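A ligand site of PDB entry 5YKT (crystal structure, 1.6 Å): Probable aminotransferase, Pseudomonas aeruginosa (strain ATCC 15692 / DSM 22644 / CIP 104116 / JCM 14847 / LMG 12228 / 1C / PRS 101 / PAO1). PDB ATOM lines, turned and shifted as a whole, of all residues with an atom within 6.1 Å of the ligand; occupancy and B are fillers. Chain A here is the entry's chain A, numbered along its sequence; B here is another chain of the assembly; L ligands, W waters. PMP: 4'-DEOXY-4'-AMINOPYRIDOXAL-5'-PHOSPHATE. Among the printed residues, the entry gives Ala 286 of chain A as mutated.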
ATOM      1  N   TRP A  49     -27.415 -12.199  -1.719  1.00  0.00           N
ATOM      2  CA  TRP A  49     -28.147 -10.990  -2.126  1.00  0.00           C
ATOM      3  C   TRP A  49     -28.055 -10.794  -3.644  1.00  0.00           C
ATOM      4  O   TRP A  49     -28.953 -10.202  -4.249  1.00  0.00           O
ATOM      5  CB  TRP A  49     -27.610  -9.746  -1.467  1.00  0.00           C
ATOM      6  CG  TRP A  49     -27.549  -9.704   0.015  1.00  0.00           C
ATOM      7  CD1 TRP A  49     -27.976 -10.641   0.917  1.00  0.00           C
ATOM      8  CD2 TRP A  49     -27.059  -8.621   0.784  1.00  0.00           C
ATOM      9  NE1 TRP A  49     -27.753 -10.214   2.201  1.00  0.00           N
ATOM     10  CE2 TRP A  49     -27.179  -8.969   2.153  1.00  0.00           C
ATOM     11  CE3 TRP A  49     -26.505  -7.375   0.449  1.00  0.00           C
ATOM     12  CZ2 TRP A  49     -26.772  -8.103   3.176  1.00  0.00           C
ATOM     13  CZ3 TRP A  49     -26.105  -6.529   1.464  1.00  0.00           C
ATOM     14  CH2 TRP A  49     -26.243  -6.895   2.806  1.00  0.00           C
ATOM     15  N   ASP A  84     -24.466  -1.083  -4.715  1.00  0.00           N
ATOM     16  CA  ASP A  84     -25.409  -0.833  -3.634  1.00  0.00           C
ATOM     17  C   ASP A  84     -24.812   0.111  -2.592  1.00  0.00           C
ATOM     18  O   ASP A  84     -24.871  -0.142  -1.395  1.00  0.00           O
ATOM     19  CB  ASP A  84     -25.907  -2.142  -3.013  1.00  0.00           C
ATOM     20  CG  ASP A  84     -27.115  -1.938  -2.108  1.00  0.00           C
ATOM     21  OD1 ASP A  84     -27.996  -1.111  -2.460  1.00  0.00           O
ATOM     22  OD2 ASP A  84     -27.168  -2.610  -1.048  1.00  0.00           O
ATOM     23  N   SER A  85     -24.234   1.210  -3.093  1.00  0.00           N
ATOM     24  CA  SER A  85     -23.568   2.256  -2.309  1.00  0.00           C
ATOM     25  C   SER A  85     -22.143   1.950  -1.854  1.00  0.00           C
ATOM     26  O   SER A  85     -21.440   2.851  -1.427  1.00  0.00           O
ATOM     27  CB  SER A  85     -24.442   2.732  -1.133  1.00  0.00           C
ATOM     28  OG  SER A  85     -25.769   2.899  -1.565  1.00  0.00           O
ATOM     29  N   SER A 138     -16.359  -3.785   8.598  1.00  0.00           N
ATOM     30  CA  SER A 138     -17.697  -3.525   8.067  1.00  0.00           C
ATOM     31  C   SER A 138     -18.472  -2.569   8.970  1.00  0.00           C
ATOM     32  O   SER A 138     -18.219  -2.475  10.173  1.00  0.00           O
ATOM     33  CB  SER A 138     -18.508  -4.807   7.931  1.00  0.00           C
ATOM     34  OG  SER A 138     -18.854  -5.326   9.217  1.00  0.00           O
ATOM     35  N   ALA A 139     -19.456  -1.904   8.379  1.00  0.00           N
ATOM     36  CA  ALA A 139     -20.347  -1.046   9.169  1.00  0.00           C
ATOM     37  C   ALA A 139     -21.121  -1.868  10.196  1.00  0.00           C
ATOM     38  O   ALA A 139     -21.349  -1.415  11.308  1.00  0.00           O
ATOM     39  CB  ALA A 139     -21.307  -0.280   8.269  1.00  0.00           C
ATOM     40  N   THR A 140     -21.525  -3.096   9.832  1.00  0.00           N
ATOM     41  CA  THR A 140     -22.158  -3.991  10.804  1.00  0.00           C
ATOM     42  C   THR A 140     -21.290  -4.120  12.041  1.00  0.00           C
ATOM     43  O   THR A 140     -21.777  -3.958  13.180  1.00  0.00           O
ATOM     44  CB  THR A 140     -22.412  -5.389  10.221  1.00  0.00           C
ATOM     45  OG1 THR A 140     -23.422  -5.330   9.196  1.00  0.00           O
ATOM     46  CG2 THR A 140     -22.821  -6.351  11.297  1.00  0.00           C
ATOM     47  N   ASP A 141     -20.004  -4.414  11.836  1.00  0.00           N
ATOM     48  CA  ASP A 141     -19.118  -4.613  12.971  1.00  0.00           C
ATOM     49  C   ASP A 141     -18.915  -3.338  13.760  1.00  0.00           C
ATOM     50  O   ASP A 141     -18.857  -3.391  14.996  1.00  0.00           O
ATOM     51  CB  ASP A 141     -17.771  -5.162  12.514  1.00  0.00           C
ATOM     52  CG  ASP A 141     -17.833  -6.608  12.150  1.00  0.00           C
ATOM     53  OD1 ASP A 141     -18.900  -7.266  12.287  1.00  0.00           O
ATOM     54  OD2 ASP A 141     -16.773  -7.104  11.726  1.00  0.00           O
ATOM     55  N   ASN A 143     -21.130  -1.028  14.230  1.00  0.00           N
ATOM     56  CA  ASN A 143     -22.338  -0.970  15.060  1.00  0.00           C
ATOM     57  C   ASN A 143     -22.308  -1.988  16.218  1.00  0.00           C
ATOM     58  O   ASN A 143     -22.591  -1.617  17.376  1.00  0.00           O
ATOM     59  CB  ASN A 143     -23.593  -1.130  14.196  1.00  0.00           C
ATOM     60  CG  ASN A 143     -23.915   0.105  13.392  1.00  0.00           C
ATOM     61  OD1 ASN A 143     -23.663   1.235  13.843  1.00  0.00           O
ATOM     62  ND2 ASN A 143     -24.497  -0.091  12.199  1.00  0.00           N
ATOM     63  N   TYR A 166     -32.245  -0.324   9.092  1.00  0.00           N
ATOM     64  CA  TYR A 166     -31.240  -1.344   8.778  1.00  0.00           C
ATOM     65  C   TYR A 166     -29.892  -0.844   9.223  1.00  0.00           C
ATOM     66  O   TYR A 166     -29.502   0.274   8.885  1.00  0.00           O
ATOM     67  CB  TYR A 166     -31.173  -1.730   7.300  1.00  0.00           C
ATOM     68  CG  TYR A 166     -30.303  -2.954   7.061  1.00  0.00           C
ATOM     69  CD1 TYR A 166     -30.664  -4.189   7.592  1.00  0.00           C
ATOM     70  CD2 TYR A 166     -29.116  -2.887   6.362  1.00  0.00           C
ATOM     71  CE1 TYR A 166     -29.883  -5.318   7.387  1.00  0.00           C
ATOM     72  CE2 TYR A 166     -28.306  -4.016   6.159  1.00  0.00           C
ATOM     73  CZ  TYR A 166     -28.702  -5.222   6.683  1.00  0.00           C
ATOM     74  OH  TYR A 166     -27.899  -6.339   6.481  1.00  0.00           O
ATOM     75  N   HIS A 167     -29.190  -1.668   9.994  1.00  0.00           N
ATOM     76  CA  HIS A 167     -27.845  -1.351  10.471  1.00  0.00           C
ATOM     77  C   HIS A 167     -26.852  -2.478  10.206  1.00  0.00           C
ATOM     78  O   HIS A 167     -25.782  -2.470  10.794  1.00  0.00           O
ATOM     79  CB  HIS A 167     -27.900  -1.049  11.973  1.00  0.00           C
ATOM     80  CG  HIS A 167     -28.720   0.145  12.284  1.00  0.00           C
ATOM     81  ND1 HIS A 167     -28.315   1.411  11.941  1.00  0.00           N
ATOM     82  CD2 HIS A 167     -29.977   0.263  12.753  1.00  0.00           C
ATOM     83  CE1 HIS A 167     -29.283   2.274  12.229  1.00  0.00           C
ATOM     84  NE2 HIS A 167     -30.295   1.601  12.737  1.00  0.00           N
ATOM     85  N   GLY A 168     -27.194  -3.406   9.313  1.00  0.00           N
ATOM     86  CA  GLY A 168     -26.379  -4.580   9.055  1.00  0.00           C
ATOM     87  C   GLY A 168     -26.866  -5.795   9.784  1.00  0.00           C
ATOM     88  O   GLY A 168     -27.986  -5.835  10.301  1.00  0.00           O
ATOM     89  N   SER A 169     -25.999  -6.805   9.853  1.00  0.00           N
ATOM     90  CA  SER A 169     -26.332  -8.067  10.530  1.00  0.00           C
ATOM     91  C   SER A 169     -26.081  -7.947  12.032  1.00  0.00           C
ATOM     92  O   SER A 169     -25.304  -8.708  12.623  1.00  0.00           O
ATOM     93  CB  SER A 169     -25.611  -9.239   9.867  1.00  0.00           C
ATOM     94  OG  SER A 169     -24.194  -9.009   9.780  1.00  0.00           O
ATOM     95  N   GLU A 226     -29.960   5.832  11.848  1.00  0.00           N
ATOM     96  CA  GLU A 226     -29.568   6.760  10.796  1.00  0.00           C
ATOM     97  C   GLU A 226     -30.179   8.125  11.142  1.00  0.00           C
ATOM     98  O   GLU A 226     -31.231   8.179  11.772  1.00  0.00           O
ATOM     99  CB  GLU A 226     -30.106   6.339   9.457  1.00  0.00           C
ATOM    100  CG  GLU A 226     -29.588   5.029   8.907  1.00  0.00           C
ATOM    101  CD  GLU A 226     -30.105   4.801   7.509  1.00  0.00           C
ATOM    102  OE1 GLU A 226     -29.411   5.247   6.567  1.00  0.00           O
ATOM    103  OE2 GLU A 226     -31.221   4.251   7.369  1.00  0.00           O
ATOM    104  N   THR A 230     -32.973   5.507   5.401  1.00  0.00           N
ATOM    105  CA  THR A 230     -32.771   5.224   3.985  1.00  0.00           C
ATOM    106  C   THR A 230     -33.022   3.783   3.580  1.00  0.00           C
ATOM    107  O   THR A 230     -32.880   3.461   2.411  1.00  0.00           O
ATOM    108  CB  THR A 230     -31.339   5.601   3.533  1.00  0.00           C
ATOM    109  OG1 THR A 230     -30.397   4.739   4.186  1.00  0.00           O
ATOM    110  CG2 THR A 230     -31.050   7.050   3.838  1.00  0.00           C
ATOM    111  N   ASN A 231     -33.423   2.902   4.512  1.00  0.00           N
ATOM    112  CA  ASN A 231     -33.549   1.491   4.209  1.00  0.00           C
ATOM    113  C   ASN A 231     -34.987   0.980   4.225  1.00  0.00           C
ATOM    114  O   ASN A 231     -35.230  -0.205   4.376  1.00  0.00           O
ATOM    115  CB  ASN A 231     -32.653   0.720   5.173  1.00  0.00           C
ATOM    116  CG  ASN A 231     -31.196   0.791   4.763  1.00  0.00           C
ATOM    117  OD1 ASN A 231     -30.853   0.323   3.697  1.00  0.00           O
ATOM    118  ND2 ASN A 231     -30.343   1.364   5.588  1.00  0.00           N
ATOM    119  N   ASP A 259     -25.566   6.526  12.528  1.00  0.00           N
ATOM    120  CA  ASP A 259     -25.040   5.640  11.483  1.00  0.00           C
ATOM    121  C   ASP A 259     -25.220   6.328  10.126  1.00  0.00           C
ATOM    122  O   ASP A 259     -26.357   6.468   9.636  1.00  0.00           O
ATOM    123  CB  ASP A 259     -25.794   4.322  11.553  1.00  0.00           C
ATOM    124  CG  ASP A 259     -25.340   3.304  10.519  1.00  0.00           C
ATOM    125  OD1 ASP A 259     -24.535   3.617   9.608  1.00  0.00           O
ATOM    126  OD2 ASP A 259     -25.819   2.146  10.613  1.00  0.00           O
ATOM    127  N   GLU A 260     -24.101   6.762   9.542  1.00  0.00           N
ATOM    128  CA  GLU A 260     -24.081   7.533   8.311  1.00  0.00           C
ATOM    129  C   GLU A 260     -23.614   6.721   7.091  1.00  0.00           C
ATOM    130  O   GLU A 260     -23.238   7.295   6.057  1.00  0.00           O
ATOM    131  CB  GLU A 260     -23.224   8.782   8.490  1.00  0.00           C
ATOM    132  CG  GLU A 260     -23.839   9.749   9.492  1.00  0.00           C
ATOM    133  CD  GLU A 260     -24.085  11.146   8.923  1.00  0.00           C
ATOM    134  OE1 GLU A 260     -24.418  11.260   7.728  1.00  0.00           O
ATOM    135  OE2 GLU A 260     -24.003  12.097   9.716  1.00  0.00           O
ATOM    136  N   THR A 261     -23.710   5.411   7.189  1.00  0.00           N
ATOM    137  CA  THR A 261     -23.316   4.514   6.112  1.00  0.00           C
ATOM    138  C   THR A 261     -23.945   4.907   4.768  1.00  0.00           C
ATOM    139  O   THR A 261     -23.257   4.811   3.743  1.00  0.00           O
ATOM    140  CB  THR A 261     -23.648   3.068   6.507  1.00  0.00           C
ATOM    141  OG1 THR A 261     -22.834   2.729   7.647  1.00  0.00           O
ATOM    142  CG2 THR A 261     -23.349   2.067   5.389  1.00  0.00           C
ATOM    143  N   HIS A 262     -25.212   5.306   4.785  1.00  0.00           N
ATOM    144  CA  HIS A 262     -25.865   5.887   3.605  1.00  0.00           C
ATOM    145  C   HIS A 262     -25.948   7.403   3.586  1.00  0.00           C
ATOM    146  O   HIS A 262     -25.824   8.027   2.512  1.00  0.00           O
ATOM    147  CB  HIS A 262     -27.283   5.333   3.422  1.00  0.00           C
ATOM    148  CG  HIS A 262     -27.328   3.949   2.891  1.00  0.00           C
ATOM    149  ND1 HIS A 262     -28.491   3.214   2.860  1.00  0.00           N
ATOM    150  CD2 HIS A 262     -26.385   3.192   2.283  1.00  0.00           C
ATOM    151  CE1 HIS A 262     -28.243   2.042   2.305  1.00  0.00           C
ATOM    152  NE2 HIS A 262     -26.964   2.000   1.968  1.00  0.00           N
ATOM    153  N   VAL A 283     -20.830   6.350  12.989  1.00  0.00           N
ATOM    154  CA  VAL A 283     -20.463   5.127  12.256  1.00  0.00           C
ATOM    155  C   VAL A 283     -20.508   5.415  10.755  1.00  0.00           C
ATOM    156  O   VAL A 283     -21.473   5.990  10.258  1.00  0.00           O
ATOM    157  CB  VAL A 283     -21.382   3.946  12.617  1.00  0.00           C
ATOM    158  CG1 VAL A 283     -21.146   2.749  11.699  1.00  0.00           C
ATOM    159  CG2 VAL A 283     -21.169   3.546  14.069  1.00  0.00           C
ATOM    160  N   GLY A 285     -19.529   3.343   6.957  1.00  0.00           N
ATOM    161  CA  GLY A 285     -19.117   2.130   6.265  1.00  0.00           C
ATOM    162  C   GLY A 285     -18.143   2.236   5.087  1.00  0.00           C
ATOM    163  O   GLY A 285     -17.336   3.167   4.986  1.00  0.00           O
ATOM    164  N   ALA A 286     -18.214   1.261   4.183  1.00  0.00           N
ATOM    165  CA  ALA A 286     -17.085   0.961   3.292  1.00  0.00           C
ATOM    166  C   ALA A 286     -16.917   1.858   2.081  1.00  0.00           C
ATOM    167  O   ALA A 286     -15.889   1.734   1.408  1.00  0.00           O
ATOM    168  CB  ALA A 286     -17.133  -0.492   2.860  1.00  0.00           C
ATOM    169  N   SER A 294     -14.510  -2.248   4.925  1.00  0.00           N
ATOM    170  CA  SER A 294     -14.016  -1.323   5.933  1.00  0.00           C
ATOM    171  C   SER A 294     -15.146  -0.544   6.558  1.00  0.00           C
ATOM    172  O   SER A 294     -16.216  -0.421   5.969  1.00  0.00           O
ATOM    173  CB  SER A 294     -13.053  -0.292   5.349  1.00  0.00           C
ATOM    174  OG  SER A 294     -12.039  -0.816   4.545  1.00  0.00           O
ATOM    175  N   GLY B 326     -25.187 -12.126   5.175  1.00  0.00           N
ATOM    176  CA  GLY B 326     -24.585 -11.452   4.026  1.00  0.00           C
ATOM    177  C   GLY B 326     -24.050 -10.133   4.497  1.00  0.00           C
ATOM    178  O   GLY B 326     -24.191  -9.794   5.662  1.00  0.00           O
ATOM    179  N   GLY B 327     -23.488  -9.363   3.590  1.00  0.00           N
ATOM    180  CA  GLY B 327     -23.005  -8.021   3.872  1.00  0.00           C
ATOM    181  C   GLY B 327     -22.702  -7.298   2.586  1.00  0.00           C
ATOM    182  O   GLY B 327     -22.523  -7.936   1.536  1.00  0.00           O
ATOM    183  N   THR B 328     -22.699  -5.971   2.631  1.00  0.00           N
ATOM    184  CA  THR B 328     -22.693  -5.176   1.401  1.00  0.00           C
ATOM    185  C   THR B 328     -21.479  -5.393   0.513  1.00  0.00           C
ATOM    186  O   THR B 328     -21.607  -5.405  -0.729  1.00  0.00           O
ATOM    187  CB  THR B 328     -22.891  -3.692   1.740  1.00  0.00           C
ATOM    188  OG1 THR B 328     -24.074  -3.554   2.538  1.00  0.00           O
ATOM    189  CG2 THR B 328     -23.031  -2.835   0.483  1.00  0.00           C
ATOM    190  N   LEU B 329     -20.311  -5.606   1.112  1.00  0.00           N
ATOM    191  CA  LEU B 329     -19.078  -5.815   0.325  1.00  0.00           C
ATOM    192  C   LEU B 329     -18.669  -7.286   0.277  1.00  0.00           C
ATOM    193  O   LEU B 329     -17.592  -7.599  -0.243  1.00  0.00           O
ATOM    194  CB  LEU B 329     -17.931  -4.934   0.855  1.00  0.00           C
ATOM    195  CG  LEU B 329     -17.946  -3.524   0.247  1.00  0.00           C
ATOM    196  CD1 LEU B 329     -19.056  -2.667   0.811  1.00  0.00           C
ATOM    197  CD2 LEU B 329     -16.594  -2.869   0.443  1.00  0.00           C
HETATM  198  N1  PMP L   1     -25.818   0.804   8.320  1.00  0.00           N
HETATM  199  C2  PMP L   1     -26.632   1.198   7.318  1.00  0.00           C
HETATM  200  C2A PMP L   1     -27.446   2.457   7.426  1.00  0.00           C
HETATM  201  C3  PMP L   1     -26.698   0.404   6.086  1.00  0.00           C
HETATM  202  O3  PMP L   1     -27.502   0.755   5.058  1.00  0.00           O
HETATM  203  C4  PMP L   1     -25.912  -0.831   5.977  1.00  0.00           C
HETATM  204  C4A PMP L   1     -25.989  -1.639   4.713  1.00  0.00           C
HETATM  205  N4A PMP L   1     -25.743  -0.787   3.565  1.00  0.00           N
HETATM  206  C5  PMP L   1     -25.065  -1.159   7.139  1.00  0.00           C
HETATM  207  C6  PMP L   1     -25.086  -0.324   8.250  1.00  0.00           C
HETATM  208  C5A PMP L   1     -24.234  -2.427   7.138  1.00  0.00           C
HETATM  209  O4P PMP L   1     -23.177  -2.350   6.193  1.00  0.00           O
HETATM  210  P   PMP L   1     -22.462  -3.735   5.803  1.00  0.00           P
HETATM  211  O1P PMP L   1     -23.444  -4.557   5.045  1.00  0.00           O
HETATM  212  O2P PMP L   1     -22.023  -4.306   7.137  1.00  0.00           O
HETATM  213  O3P PMP L   1     -21.328  -3.288   4.936  1.00  0.00           O
HETATM  214  O   HOH W   1     -28.939  -1.246   3.195  1.00  0.00           O
HETATM  215  O   HOH W   2     -19.248  -1.610   5.524  1.00  0.00           O
HETATM  216  O   HOH W   3     -21.269  -6.890   7.323  1.00  0.00           O
HETATM  217  O   HOH W   4     -25.326  -6.101   6.205  1.00  0.00           O
HETATM  218  O   HOH W   5     -26.556  -2.992   1.855  1.00  0.00           O
HETATM  219  O   HOH W   6     -22.419  -0.733   3.666  1.00  0.00           O
HETATM  220  O   HOH W   7     -19.668  -5.224   3.926  1.00  0.00           O
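A nitrogen (N1) of the ligand sits at hydrogen-bond distance from the side-chain carboxylate (OD2) of Asp 259. N of Thr 140 sits at hydrogen-bond distance from O2P of the ligand (3.0 Å). The side-chain hydroxyl (OG1) of Thr 140 sits at hydrogen-bond distance from an oxygen (O2P) of the ligand, 2.7 Å away. An oxygen (O1P) of the ligand sits at hydrogen-bond distance from the backbone NH of Thr 328 of chain B (2.9 Å). The side-chain hydroxyl of Thr 328 of chain B lies within hydrogen-bond range of an oxygen (O1P) of the ligand, 2.8 Å away. ND2 of Asn 231 lies within hydrogen-bond range of O3 of the ligand (3.0 Å). NE2 of His 262 sits close to O3 of the ligand (3.4 Å).
OD2 of Asp 259 sits at hydrogen-bond distance from ND1 of His 167 (2.9 Å). OD1 of Asp 259 is in hydrogen-bond range of OG1 of Thr 261 (2.7 Å). OD2 of Asp 259 is in hydrogen-bond range of ND2 of Asn 143 (3.0 Å). The backbone NH (N) of Ser 169 is in hydrogen-bond range of the side-chain hydroxyl (OG1) of Thr 140 (3.0 Å). The side-chain hydroxyl of Thr 230 is in hydrogen-bond range of a ring nitrogen (ND1) of His 262 (2.8 Å). O of His 167 is in hydrogen-bond range of ND2 of Asn 143 (3.0 Å). OE1 of Glu 226 is in hydrogen-bond range of OG1 of Thr 230, 2.6 Å away. N of Gly 285 is in hydrogen-bond range of OG1 of Thr 261 (3.4 Å).
Ser 138 touches the ligand. Ala 139 touches the ligand (CB to O4P, 3.5 Å). Asn 143 touches the ligand (ND2 to C6, 3.999 Å). Tyr 166 touches the ligand (O to C2A, 3.3 Å). His 167 touches the ligand. CA of Gly 168 touches C5A of the ligand, at 3.6 Å. OE1 of Glu 226 touches C2A of the ligand, 3.5 Å away. CB of Thr 261 touches C2 of the ligand, 3.6 Å away. Gly 327 of chain B touches the ligand. Hydrophobic or aromatic side chains within 4 Å of the ligand: Ala 139, Tyr 166 and His 262.
Water W4 lies within hydrogen-bond range of OH of Tyr 166 (2.6 Å) and O1P of the ligand (2.7 Å). Water W3 lies within hydrogen-bond range of an oxygen (O2P) of the ligand (2.7 Å), the side-chain hydroxyl (OG1) of Thr 140 (3.3 Å) and the side-chain hydroxyl (OG) of Ser 138 (3.4 Å). Water W2 lies within hydrogen-bond range of an oxygen (O3P) of the ligand, the backbone NH of Ala 139, the backbone carbonyl oxygen of Ser 294 and the backbone NH of Ala 286. Water W5 lies within hydrogen-bond range of the side-chain hydroxyl (OG1) of Thr 328 of chain B (2.6 Å), a nitrogen (N4A) of the ligand (2.9 Å) and the side-chain carboxylate (OD2) of Asp 84 (3.0 Å). Water W6 bridges O3P of the ligand (3.1 Å) and OG1 of Thr 328 of chain B (3.5 Å). Water W1 lies within hydrogen-bond range of the side-chain amide oxygen of Asn 231 and an oxygen (O3) of the ligand.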
